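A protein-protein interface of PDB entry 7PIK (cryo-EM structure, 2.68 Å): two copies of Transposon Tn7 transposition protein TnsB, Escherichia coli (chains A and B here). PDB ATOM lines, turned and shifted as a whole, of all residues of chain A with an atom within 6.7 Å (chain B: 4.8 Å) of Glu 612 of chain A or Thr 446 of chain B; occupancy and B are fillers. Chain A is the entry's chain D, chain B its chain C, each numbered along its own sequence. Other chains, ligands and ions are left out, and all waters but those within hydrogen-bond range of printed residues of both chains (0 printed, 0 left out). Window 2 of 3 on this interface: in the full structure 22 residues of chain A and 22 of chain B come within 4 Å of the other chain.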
ATOM      1  N   LYS A 607       5.711 -16.538  11.352  1.00  0.00           N
ATOM      2  CA  LYS A 607       6.498 -17.767  11.311  1.00  0.00           C
ATOM      3  C   LYS A 607       5.938 -18.747  10.289  1.00  0.00           C
ATOM      4  O   LYS A 607       6.683 -19.289   9.461  1.00  0.00           O
ATOM      5  CB  LYS A 607       6.548 -18.405  12.698  1.00  0.00           C
ATOM      6  N   ARG A 608       4.621 -18.969  10.313  1.00  0.00           N
ATOM      7  CA  ARG A 608       4.002 -19.878   9.359  1.00  0.00           C
ATOM      8  C   ARG A 608       4.110 -19.344   7.939  1.00  0.00           C
ATOM      9  O   ARG A 608       4.217 -20.122   6.987  1.00  0.00           O
ATOM     10  CB  ARG A 608       2.538 -20.114   9.731  1.00  0.00           C
ATOM     11  CG  ARG A 608       2.333 -20.795  11.076  1.00  0.00           C
ATOM     12  CD  ARG A 608       3.241 -21.998  11.248  1.00  0.00           C
ATOM     13  NE  ARG A 608       2.691 -22.959  12.195  1.00  0.00           N
ATOM     14  CZ  ARG A 608       2.731 -22.819  13.513  1.00  0.00           C
ATOM     15  NH1 ARG A 608       3.286 -21.761  14.080  1.00  0.00           N
ATOM     16  NH2 ARG A 608       2.198 -23.765  14.283  1.00  0.00           N
ATOM     17  N   ARG A 609       4.089 -18.019   7.769  1.00  0.00           N
ATOM     18  CA  ARG A 609       4.196 -17.449   6.431  1.00  0.00           C
ATOM     19  C   ARG A 609       5.557 -17.744   5.810  1.00  0.00           C
ATOM     20  O   ARG A 609       5.644 -18.212   4.668  1.00  0.00           O
ATOM     21  CB  ARG A 609       3.926 -15.943   6.478  1.00  0.00           C
ATOM     22  CG  ARG A 609       3.959 -15.278   5.114  1.00  0.00           C
ATOM     23  CD  ARG A 609       3.587 -13.810   5.200  1.00  0.00           C
ATOM     24  NE  ARG A 609       2.184 -13.627   5.549  1.00  0.00           N
ATOM     25  CZ  ARG A 609       1.632 -12.459   5.850  1.00  0.00           C
ATOM     26  NH1 ARG A 609       2.342 -11.343   5.864  1.00  0.00           N
ATOM     27  NH2 ARG A 609       0.336 -12.409   6.140  1.00  0.00           N
ATOM     28  N   GLU A 610       6.640 -17.487   6.552  1.00  0.00           N
ATOM     29  CA  GLU A 610       7.948 -17.843   5.997  1.00  0.00           C
ATOM     30  C   GLU A 610       8.138 -19.352   5.884  1.00  0.00           C
ATOM     31  O   GLU A 610       8.816 -19.814   4.958  1.00  0.00           O
ATOM     32  CB  GLU A 610       9.116 -17.219   6.771  1.00  0.00           C
ATOM     33  CG  GLU A 610       9.418 -15.760   6.403  1.00  0.00           C
ATOM     34  CD  GLU A 610       8.775 -14.743   7.306  1.00  0.00           C
ATOM     35  OE1 GLU A 610       8.235 -15.144   8.346  1.00  0.00           O
ATOM     36  OE2 GLU A 610       8.809 -13.541   6.973  1.00  0.00           O
ATOM     37  N   LEU A 611       7.552 -20.143   6.788  1.00  0.00           N
ATOM     38  CA  LEU A 611       7.653 -21.594   6.648  1.00  0.00           C
ATOM     39  C   LEU A 611       6.981 -22.063   5.360  1.00  0.00           C
ATOM     40  O   LEU A 611       7.521 -22.904   4.627  1.00  0.00           O
ATOM     41  CB  LEU A 611       7.039 -22.279   7.871  1.00  0.00           C
ATOM     42  CG  LEU A 611       7.339 -23.764   8.100  1.00  0.00           C
ATOM     43  CD1 LEU A 611       7.317 -24.075   9.589  1.00  0.00           C
ATOM     44  CD2 LEU A 611       6.355 -24.661   7.362  1.00  0.00           C
ATOM     45  N   GLU A 612       5.797 -21.518   5.069  1.00  0.00           N
ATOM     46  CA  GLU A 612       5.097 -21.833   3.830  1.00  0.00           C
ATOM     47  C   GLU A 612       5.898 -21.398   2.613  1.00  0.00           C
ATOM     48  O   GLU A 612       5.989 -22.139   1.628  1.00  0.00           O
ATOM     49  CB  GLU A 612       3.727 -21.161   3.820  1.00  0.00           C
ATOM     50  CG  GLU A 612       2.895 -21.495   2.600  1.00  0.00           C
ATOM     51  CD  GLU A 612       1.531 -20.852   2.643  1.00  0.00           C
ATOM     52  OE1 GLU A 612       1.245 -20.130   3.619  1.00  0.00           O
ATOM     53  OE2 GLU A 612       0.754 -21.049   1.690  1.00  0.00           O
ATOM     54  N   ALA A 613       6.473 -20.195   2.656  1.00  0.00           N
ATOM     55  CA  ALA A 613       7.278 -19.737   1.530  1.00  0.00           C
ATOM     56  C   ALA A 613       8.461 -20.667   1.294  1.00  0.00           C
ATOM     57  O   ALA A 613       8.762 -21.025   0.149  1.00  0.00           O
ATOM     58  CB  ALA A 613       7.754 -18.305   1.769  1.00  0.00           C
ATOM     59  N   PHE A 614       9.122 -21.094   2.372  1.00  0.00           N
ATOM     60  CA  PHE A 614      10.271 -21.984   2.242  1.00  0.00           C
ATOM     61  C   PHE A 614       9.871 -23.329   1.644  1.00  0.00           C
ATOM     62  O   PHE A 614      10.530 -23.827   0.723  1.00  0.00           O
ATOM     63  CB  PHE A 614      10.938 -22.178   3.604  1.00  0.00           C
ATOM     64  N   ILE A 615       8.796 -23.938   2.158  1.00  0.00           N
ATOM     65  CA  ILE A 615       8.413 -25.256   1.655  1.00  0.00           C
ATOM     66  C   ILE A 615       7.942 -25.162   0.207  1.00  0.00           C
ATOM     67  O   ILE A 615       8.271 -26.019  -0.624  1.00  0.00           O
ATOM     68  CB  ILE A 615       7.358 -25.917   2.564  1.00  0.00           C
ATOM     69  CG1 ILE A 615       6.984 -27.299   2.023  1.00  0.00           C
ATOM     70  CG2 ILE A 615       6.113 -25.067   2.690  1.00  0.00           C
ATOM     71  CD1 ILE A 615       6.086 -28.093   2.943  1.00  0.00           C
ATOM     72  N   GLN A 616       7.186 -24.114  -0.128  1.00  0.00           N
ATOM     73  CA  GLN A 616       6.744 -23.926  -1.503  1.00  0.00           C
ATOM     74  C   GLN A 616       7.929 -23.761  -2.444  1.00  0.00           C
ATOM     75  O   GLN A 616       7.981 -24.379  -3.515  1.00  0.00           O
ATOM     76  CB  GLN A 616       5.822 -22.711  -1.584  1.00  0.00           C
ATOM     77  CG  GLN A 616       5.232 -22.472  -2.953  1.00  0.00           C
ATOM     78  CD  GLN A 616       4.284 -21.297  -2.969  1.00  0.00           C
ATOM     79  OE1 GLN A 616       4.087 -20.626  -1.956  1.00  0.00           O
ATOM     80  NE2 GLN A 616       3.691 -21.037  -4.125  1.00  0.00           N
ATOM     81  N   GLN A 617       8.903 -22.933  -2.051  1.00  0.00           N
ATOM     82  CA  GLN A 617      10.055 -22.692  -2.912  1.00  0.00           C
ATOM     83  C   GLN A 617      10.893 -23.951  -3.087  1.00  0.00           C
ATOM     84  O   GLN A 617      11.345 -24.245  -4.199  1.00  0.00           O
ATOM     85  CB  GLN A 617      10.902 -21.555  -2.345  1.00  0.00           C
ATOM     86  CG  GLN A 617      11.914 -21.005  -3.330  1.00  0.00           C
ATOM     87  CD  GLN A 617      11.271 -20.569  -4.632  1.00  0.00           C
ATOM     88  OE1 GLN A 617      11.403 -21.235  -5.657  1.00  0.00           O
ATOM     89  NE2 GLN A 617      10.563 -19.446  -4.594  1.00  0.00           N
ATOM     90  N   ILE B 395      -6.233 -16.639  -3.179  1.00  0.00           N
ATOM     91  CA  ILE B 395      -5.517 -17.869  -2.862  1.00  0.00           C
ATOM     92  C   ILE B 395      -4.373 -18.097  -3.843  1.00  0.00           C
ATOM     93  O   ILE B 395      -3.264 -18.474  -3.446  1.00  0.00           O
ATOM     94  CB  ILE B 395      -6.485 -19.066  -2.844  1.00  0.00           C
ATOM     95  CG1 ILE B 395      -7.531 -18.897  -1.746  1.00  0.00           C
ATOM     96  CG2 ILE B 395      -5.726 -20.370  -2.661  1.00  0.00           C
ATOM     97  CD1 ILE B 395      -8.657 -19.894  -1.837  1.00  0.00           C
ATOM     98  N   ILE B 442       0.599 -27.593  -2.911  1.00  0.00           N
ATOM     99  CA  ILE B 442       0.768 -26.161  -2.679  1.00  0.00           C
ATOM    100  C   ILE B 442      -0.570 -25.514  -2.352  1.00  0.00           C
ATOM    101  O   ILE B 442      -0.684 -24.721  -1.406  1.00  0.00           O
ATOM    102  CB  ILE B 442       1.432 -25.496  -3.899  1.00  0.00           C
ATOM    103  CG1 ILE B 442       2.864 -26.009  -4.072  1.00  0.00           C
ATOM    104  CG2 ILE B 442       1.413 -23.983  -3.763  1.00  0.00           C
ATOM    105  CD1 ILE B 442       3.561 -25.464  -5.298  1.00  0.00           C
ATOM    106  N   ILE B 443      -1.607 -25.847  -3.125  1.00  0.00           N
ATOM    107  CA  ILE B 443      -2.922 -25.252  -2.898  1.00  0.00           C
ATOM    108  C   ILE B 443      -3.476 -25.675  -1.541  1.00  0.00           C
ATOM    109  O   ILE B 443      -4.058 -24.861  -0.813  1.00  0.00           O
ATOM    110  CB  ILE B 443      -3.881 -25.617  -4.047  1.00  0.00           C
ATOM    111  CG1 ILE B 443      -3.363 -25.051  -5.368  1.00  0.00           C
ATOM    112  CG2 ILE B 443      -5.283 -25.096  -3.767  1.00  0.00           C
ATOM    113  CD1 ILE B 443      -3.231 -23.547  -5.374  1.00  0.00           C
ATOM    114  N   LEU B 444      -3.304 -26.948  -1.180  1.00  0.00           N
ATOM    115  CA  LEU B 444      -3.805 -27.427   0.104  1.00  0.00           C
ATOM    116  C   LEU B 444      -3.120 -26.722   1.266  1.00  0.00           C
ATOM    117  O   LEU B 444      -3.780 -26.302   2.224  1.00  0.00           O
ATOM    118  CB  LEU B 444      -3.612 -28.939   0.209  1.00  0.00           C
ATOM    119  CG  LEU B 444      -4.669 -29.810  -0.475  1.00  0.00           C
ATOM    120  CD1 LEU B 444      -4.335 -31.284  -0.318  1.00  0.00           C
ATOM    121  CD2 LEU B 444      -6.053 -29.508   0.077  1.00  0.00           C
ATOM    122  N   ARG B 445      -1.793 -26.575   1.199  1.00  0.00           N
ATOM    123  CA  ARG B 445      -1.083 -25.907   2.286  1.00  0.00           C
ATOM    124  C   ARG B 445      -1.441 -24.426   2.355  1.00  0.00           C
ATOM    125  O   ARG B 445      -1.557 -23.861   3.451  1.00  0.00           O
ATOM    126  CB  ARG B 445       0.422 -26.104   2.126  1.00  0.00           C
ATOM    127  CG  ARG B 445       0.867 -27.524   2.429  1.00  0.00           C
ATOM    128  CD  ARG B 445       2.375 -27.670   2.402  1.00  0.00           C
ATOM    129  NE  ARG B 445       2.784 -29.044   2.670  1.00  0.00           N
ATOM    130  CZ  ARG B 445       2.899 -29.568   3.883  1.00  0.00           C
ATOM    131  NH1 ARG B 445       2.646 -28.857   4.970  1.00  0.00           N
ATOM    132  NH2 ARG B 445       3.277 -30.837   4.009  1.00  0.00           N
ATOM    133  N   THR B 446      -1.631 -23.783   1.200  1.00  0.00           N
ATOM    134  CA  THR B 446      -2.071 -22.393   1.196  1.00  0.00           C
ATOM    135  C   THR B 446      -3.444 -22.247   1.843  1.00  0.00           C
ATOM    136  O   THR B 446      -3.673 -21.320   2.628  1.00  0.00           O
ATOM    137  CB  THR B 446      -2.096 -21.854  -0.233  1.00  0.00           C
ATOM    138  OG1 THR B 446      -0.840 -22.125  -0.867  1.00  0.00           O
ATOM    139  CG2 THR B 446      -2.345 -20.355  -0.234  1.00  0.00           C
ATOM    140  N   ILE B 447      -4.368 -23.156   1.523  1.00  0.00           N
ATOM    141  CA  ILE B 447      -5.700 -23.114   2.121  1.00  0.00           C
ATOM    142  C   ILE B 447      -5.610 -23.318   3.626  1.00  0.00           C
ATOM    143  O   ILE B 447      -6.285 -22.630   4.402  1.00  0.00           O
ATOM    144  CB  ILE B 447      -6.616 -24.161   1.457  1.00  0.00           C
ATOM    145  CG1 ILE B 447      -7.062 -23.685   0.075  1.00  0.00           C
ATOM    146  CG2 ILE B 447      -7.826 -24.456   2.331  1.00  0.00           C
ATOM    147  CD1 ILE B 447      -7.816 -24.732  -0.709  1.00  0.00           C
ATOM    148  N   LEU B 448      -4.781 -24.269   4.061  1.00  0.00           N
ATOM    149  CA  LEU B 448      -4.615 -24.519   5.490  1.00  0.00           C
ATOM    150  C   LEU B 448      -4.104 -23.276   6.211  1.00  0.00           C
ATOM    151  O   LEU B 448      -4.637 -22.886   7.258  1.00  0.00           O
ATOM    152  CB  LEU B 448      -3.663 -25.695   5.703  1.00  0.00           C
ATOM    153  CG  LEU B 448      -4.212 -27.087   5.390  1.00  0.00           C
ATOM    154  CD1 LEU B 448      -3.083 -28.080   5.182  1.00  0.00           C
ATOM    155  CD2 LEU B 448      -5.118 -27.548   6.508  1.00  0.00           C
ATOM    156  N   PHE B 449      -3.071 -22.633   5.655  1.00  0.00           N
ATOM    157  CA  PHE B 449      -2.533 -21.431   6.285  1.00  0.00           C
ATOM    158  C   PHE B 449      -3.564 -20.309   6.317  1.00  0.00           C
ATOM    159  O   PHE B 449      -3.725 -19.635   7.340  1.00  0.00           O
ATOM    160  CB  PHE B 449      -1.272 -20.965   5.560  1.00  0.00           C
ATOM    161  CG  PHE B 449      -0.841 -19.576   5.938  1.00  0.00           C
ATOM    162  CD1 PHE B 449      -0.297 -19.322   7.185  1.00  0.00           C
ATOM    163  CD2 PHE B 449      -1.001 -18.520   5.057  1.00  0.00           C
ATOM    164  CE1 PHE B 449       0.090 -18.048   7.542  1.00  0.00           C
ATOM    165  CE2 PHE B 449      -0.614 -17.242   5.409  1.00  0.00           C
ATOM    166  CZ  PHE B 449      -0.069 -17.007   6.652  1.00  0.00           C
ATOM    167  N   ARG B 450      -4.271 -20.094   5.204  1.00  0.00           N
ATOM    168  CA  ARG B 450      -5.246 -19.009   5.141  1.00  0.00           C
ATOM    169  C   ARG B 450      -6.395 -19.240   6.115  1.00  0.00           C
ATOM    170  O   ARG B 450      -6.918 -18.287   6.705  1.00  0.00           O
ATOM    171  CB  ARG B 450      -5.756 -18.861   3.705  1.00  0.00           C
ATOM    172  CG  ARG B 450      -6.678 -17.672   3.443  1.00  0.00           C
ATOM    173  CD  ARG B 450      -8.143 -18.046   3.624  1.00  0.00           C
ATOM    174  NE  ARG B 450      -9.048 -16.972   3.234  1.00  0.00           N
ATOM    175  CZ  ARG B 450     -10.355 -16.981   3.454  1.00  0.00           C
ATOM    176  NH1 ARG B 450     -10.946 -17.994   4.068  1.00  0.00           N
ATOM    177  NH2 ARG B 450     -11.089 -15.948   3.051  1.00  0.00           N
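OE2 of Glu 612 of chain A sits close to OG1 of Thr 446 of chain B (3.2 Å).
O of Ile 442 of chain B is in hydrogen-bond range of OG1 of Thr 446 of chain B (2.7 Å).
CB of Arg 608 of chain A touches CE1 of Phe 449 of chain B, at 3.9 Å.
OE1 of Glu 612 of chain A touches CD2 of Phe 449 of chain B (3.1 Å).
Ile 615 of chain A touches Arg 445 of chain B (CD1 to NE, 3.4 Å).
Gln 616 of chain A touches Ile 442 of chain B (NE2 to CG2, 3.7 Å).
Lys 607 of chain A touches none of the printed residues of chain B.
Printed residues of chain B within 4 Å of Arg 608 of chain A: Phe 449.
Glu 612 of chain A touches just these residues of chain B: Thr 446 and Phe 449.
Ala 613 of chain A touches none of the printed residues of chain B.
Printed residues of chain B within 4 Å of Ile 615 of chain A: Arg 445.
Of the printed residues of chain A, Ile 442 of chain B touches Gln 616.
Of the printed residues of chain A, Arg 445 of chain B touches Ile 615 (3.4 Å).
Thr 446 of chain B touches just one residue of chain A: Glu 612.
Printed residues of chain A within 4 Å of Phe 449 of chain B: Arg 608 and Glu 612.
The nearest residue of chain A that does not touch Thr 446 of chain B is Gln 616 of chain A (5.3 Å).
The nearest printed residue of chain B that does not touch Arg 608 of chain A is Arg 445 of chain B (7.7 Å).
Of the 11 printed residues of chain A, 4 touch a printed residue of chain B.
Printed residues of chain A that touch a printed residue of chain B: Arg 608, Glu 612, Ile 615 and Gln 616.
No position is printed for both chains.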
